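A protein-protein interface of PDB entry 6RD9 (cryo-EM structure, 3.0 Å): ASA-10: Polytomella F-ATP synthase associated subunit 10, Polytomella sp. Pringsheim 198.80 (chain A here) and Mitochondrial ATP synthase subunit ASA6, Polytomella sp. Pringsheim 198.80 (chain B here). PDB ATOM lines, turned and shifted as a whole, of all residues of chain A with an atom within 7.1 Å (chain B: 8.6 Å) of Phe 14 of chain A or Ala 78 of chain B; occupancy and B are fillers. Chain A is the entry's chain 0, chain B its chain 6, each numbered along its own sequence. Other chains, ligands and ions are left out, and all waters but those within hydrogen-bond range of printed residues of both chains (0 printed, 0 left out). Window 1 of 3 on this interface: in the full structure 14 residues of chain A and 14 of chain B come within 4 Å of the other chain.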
ATOM      1  N   PHE A  12     -16.764 -16.961 -18.900  1.00  0.00           N
ATOM      2  CA  PHE A  12     -16.467 -17.122 -17.492  1.00  0.00           C
ATOM      3  C   PHE A  12     -15.673 -15.932 -16.993  1.00  0.00           C
ATOM      4  O   PHE A  12     -14.919 -15.304 -17.732  1.00  0.00           O
ATOM      5  CB  PHE A  12     -15.680 -18.401 -17.261  1.00  0.00           C
ATOM      6  CG  PHE A  12     -15.442 -18.727 -15.825  1.00  0.00           C
ATOM      7  CD1 PHE A  12     -16.399 -19.367 -15.090  1.00  0.00           C
ATOM      8  CD2 PHE A  12     -14.244 -18.420 -15.223  1.00  0.00           C
ATOM      9  CE1 PHE A  12     -16.170 -19.672 -13.788  1.00  0.00           C
ATOM     10  CE2 PHE A  12     -14.023 -18.720 -13.928  1.00  0.00           C
ATOM     11  CZ  PHE A  12     -14.979 -19.343 -13.209  1.00  0.00           C
ATOM     12  N   GLN A  13     -15.870 -15.614 -15.725  1.00  0.00           N
ATOM     13  CA  GLN A  13     -15.118 -14.573 -15.063  1.00  0.00           C
ATOM     14  C   GLN A  13     -15.065 -14.938 -13.593  1.00  0.00           C
ATOM     15  O   GLN A  13     -16.036 -15.457 -13.046  1.00  0.00           O
ATOM     16  CB  GLN A  13     -15.775 -13.221 -15.277  1.00  0.00           C
ATOM     17  CG  GLN A  13     -14.823 -12.103 -15.467  1.00  0.00           C
ATOM     18  CD  GLN A  13     -15.515 -10.902 -16.013  1.00  0.00           C
ATOM     19  OE1 GLN A  13     -16.640 -10.996 -16.491  1.00  0.00           O
ATOM     20  NE2 GLN A  13     -14.865  -9.752 -15.928  1.00  0.00           N
ATOM     21  N   PHE A  14     -13.931 -14.679 -12.964  1.00  0.00           N
ATOM     22  CA  PHE A  14     -13.766 -14.988 -11.564  1.00  0.00           C
ATOM     23  C   PHE A  14     -14.575 -14.003 -10.732  1.00  0.00           C
ATOM     24  O   PHE A  14     -15.041 -12.991 -11.251  1.00  0.00           O
ATOM     25  CB  PHE A  14     -12.294 -14.917 -11.192  1.00  0.00           C
ATOM     26  CG  PHE A  14     -11.517 -16.111 -11.598  1.00  0.00           C
ATOM     27  CD1 PHE A  14     -11.984 -17.373 -11.335  1.00  0.00           C
ATOM     28  CD2 PHE A  14     -10.311 -15.976 -12.238  1.00  0.00           C
ATOM     29  CE1 PHE A  14     -11.264 -18.468 -11.711  1.00  0.00           C
ATOM     30  CE2 PHE A  14      -9.598 -17.071 -12.615  1.00  0.00           C
ATOM     31  CZ  PHE A  14     -10.074 -18.312 -12.349  1.00  0.00           C
ATOM     32  N   PRO A  15     -14.791 -14.289  -9.449  1.00  0.00           N
ATOM     33  CA  PRO A  15     -15.340 -13.267  -8.571  1.00  0.00           C
ATOM     34  C   PRO A  15     -14.419 -12.069  -8.484  1.00  0.00           C
ATOM     35  O   PRO A  15     -13.215 -12.151  -8.699  1.00  0.00           O
ATOM     36  CB  PRO A  15     -15.462 -13.988  -7.243  1.00  0.00           C
ATOM     37  CG  PRO A  15     -15.782 -15.309  -7.639  1.00  0.00           C
ATOM     38  CD  PRO A  15     -14.967 -15.610  -8.841  1.00  0.00           C
ATOM     39  N   ALA A  16     -15.018 -10.929  -8.196  1.00  0.00           N
ATOM     40  CA  ALA A  16     -14.394  -9.661  -8.509  1.00  0.00           C
ATOM     41  C   ALA A  16     -13.309  -9.241  -7.552  1.00  0.00           C
ATOM     42  O   ALA A  16     -12.982  -8.061  -7.530  1.00  0.00           O
ATOM     43  CB  ALA A  16     -15.440  -8.579  -8.557  1.00  0.00           C
ATOM     44  N   GLY A  17     -12.792 -10.116  -6.722  1.00  0.00           N
ATOM     45  CA  GLY A  17     -11.589  -9.765  -6.015  1.00  0.00           C
ATOM     46  C   GLY A  17     -10.806 -10.984  -5.634  1.00  0.00           C
ATOM     47  O   GLY A  17     -10.075 -10.952  -4.651  1.00  0.00           O
ATOM     48  N   LEU A  18     -10.946 -12.056  -6.411  1.00  0.00           N
ATOM     49  CA  LEU A  18     -10.439 -13.361  -6.020  1.00  0.00           C
ATOM     50  C   LEU A  18      -8.932 -13.409  -5.979  1.00  0.00           C
ATOM     51  O   LEU A  18      -8.367 -14.258  -5.298  1.00  0.00           O
ATOM     52  CB  LEU A  18     -10.938 -14.424  -6.974  1.00  0.00           C
ATOM     53  CG  LEU A  18     -10.959 -15.840  -6.445  1.00  0.00           C
ATOM     54  CD1 LEU A  18     -11.901 -15.933  -5.300  1.00  0.00           C
ATOM     55  CD2 LEU A  18     -11.366 -16.768  -7.532  1.00  0.00           C
ATOM     56  N   SER A  19      -8.271 -12.507  -6.675  1.00  0.00           N
ATOM     57  CA  SER A  19      -6.830 -12.454  -6.613  1.00  0.00           C
ATOM     58  C   SER A  19      -6.340 -11.961  -5.265  1.00  0.00           C
ATOM     59  O   SER A  19      -5.187 -12.188  -4.925  1.00  0.00           O
ATOM     60  CB  SER A  19      -6.317 -11.577  -7.739  1.00  0.00           C
ATOM     61  OG  SER A  19      -6.852 -10.275  -7.632  1.00  0.00           O
ATOM     62  N   SER B  72     -12.607 -18.742 -22.311  1.00  0.00           N
ATOM     63  CA  SER B  72     -11.878 -17.530 -21.966  1.00  0.00           C
ATOM     64  C   SER B  72     -10.523 -17.764 -21.320  1.00  0.00           C
ATOM     65  O   SER B  72     -10.237 -18.859 -20.835  1.00  0.00           O
ATOM     66  CB  SER B  72     -12.720 -16.723 -20.988  1.00  0.00           C
ATOM     67  OG  SER B  72     -13.998 -16.485 -21.525  1.00  0.00           O
ATOM     68  N   THR B  73      -9.696 -16.725 -21.262  1.00  0.00           N
ATOM     69  CA  THR B  73      -8.415 -16.824 -20.577  1.00  0.00           C
ATOM     70  C   THR B  73      -8.544 -17.071 -19.086  1.00  0.00           C
ATOM     71  O   THR B  73      -7.554 -17.436 -18.458  1.00  0.00           O
ATOM     72  CB  THR B  73      -7.598 -15.560 -20.787  1.00  0.00           C
ATOM     73  OG1 THR B  73      -6.398 -15.639 -20.010  1.00  0.00           O
ATOM     74  CG2 THR B  73      -8.387 -14.338 -20.380  1.00  0.00           C
ATOM     75  N   GLN B  74      -9.716 -16.855 -18.502  1.00  0.00           N
ATOM     76  CA  GLN B  74      -9.981 -17.205 -17.120  1.00  0.00           C
ATOM     77  C   GLN B  74     -10.771 -18.485 -16.966  1.00  0.00           C
ATOM     78  O   GLN B  74     -10.810 -19.029 -15.870  1.00  0.00           O
ATOM     79  CB  GLN B  74     -10.727 -16.079 -16.428  1.00  0.00           C
ATOM     80  CG  GLN B  74      -9.963 -14.804 -16.413  1.00  0.00           C
ATOM     81  CD  GLN B  74     -10.676 -13.725 -15.672  1.00  0.00           C
ATOM     82  OE1 GLN B  74     -10.316 -12.563 -15.756  1.00  0.00           O
ATOM     83  NE2 GLN B  74     -11.718 -14.091 -14.970  1.00  0.00           N
ATOM     84  N   ALA B  75     -11.427 -18.966 -18.006  1.00  0.00           N
ATOM     85  CA  ALA B  75     -12.019 -20.288 -17.909  1.00  0.00           C
ATOM     86  C   ALA B  75     -10.982 -21.366 -18.099  1.00  0.00           C
ATOM     87  O   ALA B  75     -11.223 -22.520 -17.749  1.00  0.00           O
ATOM     88  CB  ALA B  75     -13.122 -20.467 -18.936  1.00  0.00           C
ATOM     89  N   LYS B  76      -9.845 -21.027 -18.684  1.00  0.00           N
ATOM     90  CA  LYS B  76      -8.764 -21.985 -18.763  1.00  0.00           C
ATOM     91  C   LYS B  76      -7.962 -22.020 -17.479  1.00  0.00           C
ATOM     92  O   LYS B  76      -7.488 -23.085 -17.092  1.00  0.00           O
ATOM     93  CB  LYS B  76      -7.876 -21.660 -19.954  1.00  0.00           C
ATOM     94  CG  LYS B  76      -8.585 -21.821 -21.290  1.00  0.00           C
ATOM     95  CD  LYS B  76      -7.680 -21.477 -22.456  1.00  0.00           C
ATOM     96  CE  LYS B  76      -7.055 -20.108 -22.288  1.00  0.00           C
ATOM     97  NZ  LYS B  76      -6.371 -19.617 -23.505  1.00  0.00           N
ATOM     98  N   ILE B  77      -7.820 -20.886 -16.796  1.00  0.00           N
ATOM     99  CA  ILE B  77      -7.208 -20.884 -15.471  1.00  0.00           C
ATOM    100  C   ILE B  77      -8.094 -21.620 -14.480  1.00  0.00           C
ATOM    101  O   ILE B  77      -7.609 -22.319 -13.591  1.00  0.00           O
ATOM    102  CB  ILE B  77      -6.925 -19.441 -15.025  1.00  0.00           C
ATOM    103  CG1 ILE B  77      -5.924 -18.799 -15.956  1.00  0.00           C
ATOM    104  CG2 ILE B  77      -6.355 -19.389 -13.654  1.00  0.00           C
ATOM    105  CD1 ILE B  77      -5.726 -17.346 -15.691  1.00  0.00           C
ATOM    106  N   ALA B  78      -9.402 -21.518 -14.646  1.00  0.00           N
ATOM    107  CA  ALA B  78     -10.303 -22.165 -13.713  1.00  0.00           C
ATOM    108  C   ALA B  78     -10.340 -23.668 -13.908  1.00  0.00           C
ATOM    109  O   ALA B  78     -10.644 -24.392 -12.966  1.00  0.00           O
ATOM    110  CB  ALA B  78     -11.703 -21.595 -13.853  1.00  0.00           C
ATOM    111  N   LEU B  79     -10.066 -24.157 -15.110  1.00  0.00           N
ATOM    112  CA  LEU B  79     -10.075 -25.595 -15.334  1.00  0.00           C
ATOM    113  C   LEU B  79      -8.696 -26.212 -15.278  1.00  0.00           C
ATOM    114  O   LEU B  79      -8.575 -27.391 -14.947  1.00  0.00           O
ATOM    115  CB  LEU B  79     -10.715 -25.941 -16.674  1.00  0.00           C
ATOM    116  CG  LEU B  79     -12.189 -25.607 -16.813  1.00  0.00           C
ATOM    117  CD1 LEU B  79     -12.559 -25.492 -18.270  1.00  0.00           C
ATOM    118  CD2 LEU B  79     -13.002 -26.678 -16.144  1.00  0.00           C
ATOM    119  N   PHE B  80      -7.650 -25.473 -15.619  1.00  0.00           N
ATOM    120  CA  PHE B  80      -6.330 -26.016 -15.360  1.00  0.00           C
ATOM    121  C   PHE B  80      -5.996 -25.927 -13.890  1.00  0.00           C
ATOM    122  O   PHE B  80      -5.379 -26.841 -13.350  1.00  0.00           O
ATOM    123  CB  PHE B  80      -5.259 -25.305 -16.172  1.00  0.00           C
ATOM    124  CG  PHE B  80      -3.875 -25.808 -15.901  1.00  0.00           C
ATOM    125  CD1 PHE B  80      -2.939 -25.009 -15.262  1.00  0.00           C
ATOM    126  CD2 PHE B  80      -3.509 -27.090 -16.275  1.00  0.00           C
ATOM    127  CE1 PHE B  80      -1.656 -25.482 -15.009  1.00  0.00           C
ATOM    128  CE2 PHE B  80      -2.232 -27.568 -16.025  1.00  0.00           C
ATOM    129  CZ  PHE B  80      -1.306 -26.761 -15.395  1.00  0.00           C
ATOM    130  N   GLY B  81      -6.410 -24.852 -13.226  1.00  0.00           N
ATOM    131  CA  GLY B  81      -6.181 -24.732 -11.800  1.00  0.00           C
ATOM    132  C   GLY B  81      -7.019 -25.678 -10.971  1.00  0.00           C
ATOM    133  O   GLY B  81      -6.651 -25.998  -9.845  1.00  0.00           O
ATOM    134  N   ALA B  82      -8.157 -26.116 -11.491  1.00  0.00           N
ATOM    135  CA  ALA B  82      -8.919 -27.141 -10.799  1.00  0.00           C
ATOM    136  C   ALA B  82      -8.380 -28.521 -11.083  1.00  0.00           C
ATOM    137  O   ALA B  82      -8.531 -29.419 -10.258  1.00  0.00           O
ATOM    138  CB  ALA B  82     -10.384 -27.097 -11.193  1.00  0.00           C
ATOM    139  N   LEU B  83      -7.797 -28.726 -12.257  1.00  0.00           N
ATOM    140  CA  LEU B  83      -7.124 -29.987 -12.533  1.00  0.00           C
ATOM    141  C   LEU B  83      -5.788 -30.044 -11.826  1.00  0.00           C
ATOM    142  O   LEU B  83      -5.357 -31.110 -11.392  1.00  0.00           O
ATOM    143  CB  LEU B  83      -6.934 -30.157 -14.030  1.00  0.00           C
ATOM    144  CG  LEU B  83      -6.426 -31.506 -14.502  1.00  0.00           C
ATOM    145  CD1 LEU B  83      -7.555 -32.514 -14.484  1.00  0.00           C
ATOM    146  CD2 LEU B  83      -5.812 -31.372 -15.872  1.00  0.00           C
ATOM    147  N   SER B  84      -5.121 -28.906 -11.688  1.00  0.00           N
ATOM    148  CA  SER B  84      -3.897 -28.860 -10.904  1.00  0.00           C
ATOM    149  C   SER B  84      -4.168 -29.026  -9.422  1.00  0.00           C
ATOM    150  O   SER B  84      -3.250 -29.331  -8.665  1.00  0.00           O
ATOM    151  CB  SER B  84      -3.166 -27.552 -11.147  1.00  0.00           C
ATOM    152  OG  SER B  84      -2.095 -27.422 -10.251  1.00  0.00           O
ATOM    153  N   TRP B  85      -5.397 -28.783  -8.980  1.00  0.00           N
ATOM    154  CA  TRP B  85      -5.758 -29.013  -7.591  1.00  0.00           C
ATOM    155  C   TRP B  85      -6.204 -30.441  -7.374  1.00  0.00           C
ATOM    156  O   TRP B  85      -5.877 -31.037  -6.355  1.00  0.00           O
ATOM    157  CB  TRP B  85      -6.859 -28.049  -7.170  1.00  0.00           C
ATOM    158  CG  TRP B  85      -7.342 -28.247  -5.796  1.00  0.00           C
ATOM    159  CD1 TRP B  85      -8.495 -28.831  -5.418  1.00  0.00           C
ATOM    160  CD2 TRP B  85      -6.690 -27.836  -4.606  1.00  0.00           C
ATOM    161  NE1 TRP B  85      -8.602 -28.827  -4.063  1.00  0.00           N
ATOM    162  CE2 TRP B  85      -7.498 -28.218  -3.540  1.00  0.00           C
ATOM    163  CE3 TRP B  85      -5.493 -27.185  -4.339  1.00  0.00           C
ATOM    164  CZ2 TRP B  85      -7.150 -27.973  -2.234  1.00  0.00           C
ATOM    165  CZ3 TRP B  85      -5.153 -26.949  -3.047  1.00  0.00           C
ATOM    166  CH2 TRP B  85      -5.973 -27.336  -2.011  1.00  0.00           C
ATOM    167  N   ILE B  86      -6.939 -31.007  -8.321  1.00  0.00           N
ATOM    168  CA  ILE B  86      -7.445 -32.361  -8.153  1.00  0.00           C
ATOM    169  C   ILE B  86      -6.313 -33.368  -8.270  1.00  0.00           C
ATOM    170  O   ILE B  86      -6.276 -34.364  -7.548  1.00  0.00           O
ATOM    171  CB  ILE B  86      -8.579 -32.611  -9.161  1.00  0.00           C
ATOM    172  CG1 ILE B  86      -9.864 -31.995  -8.634  1.00  0.00           C
ATOM    173  CG2 ILE B  86      -8.804 -34.074  -9.434  1.00  0.00           C
ATOM    174  CD1 ILE B  86     -11.028 -32.162  -9.539  1.00  0.00           C
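The side-chain amide nitrogen of Gln 74 of chain B lies close to the backbone NH of Phe 14 of chain A (3.0 Å).
Of the printed residues of chain B, Phe 12 of chain A touches Ser 72 (3.8 Å), Gln 74 (3.5 Å), Ala 75 (3.7 Å) and Ala 78 (3.7 Å).
Printed residues of chain B within 4 Å of Gln 13 of chain A: Gln 74 (3.4 Å).
Phe 14 of chain A touches just these residues of chain B: Gln 74 (3.0 Å) and Ala 78 (3.8 Å).
Pro 15 of chain A touches none of the printed residues of chain B.
Of the printed residues of chain A, Ser 72 of chain B touches Phe 12.
Of the printed residues of chain A, Gln 74 of chain B touches Phe 12, Gln 13 and Phe 14.
Of the printed residues of chain A, Ala 75 of chain B touches Phe 12.
Of chain A, only Phe 12 and Phe 14 come within 4 Å of Ala 78 of chain B.
The nearest printed residue of chain A that does not touch Ala 78 of chain B is Gln 13 of chain A (7.5 Å).
Phe 12 of chain A touches Ser 72 of chain B.
Phe 12 of chain A touches Gln 74 of chain B (CD2 to O, 3.5 Å).
Ala 75 of chain B touches Phe 12 of chain A (CB to CB, 3.7 Å).
Phe 12 of chain A touches Ala 78 of chain B (CE2 to CB, 3.7 Å).
CA of Gln 13 of chain A touches NE2 of Gln 74 of chain B, at 3.4 Å.
Phe 14 of chain A touches Ala 78 of chain B (CE1 to CB, 3.8 Å).
Of the 15 printed residues of chain B, 4 touch a printed residue of chain A.
Printed residues of chain B that touch a printed residue of chain A: Ser 72, Gln 74, Ala 75 and Ala 78.
Hydrophobic or aromatic side chains of chain B that line the printed part of chain A: Ala 75 and Ala 78.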
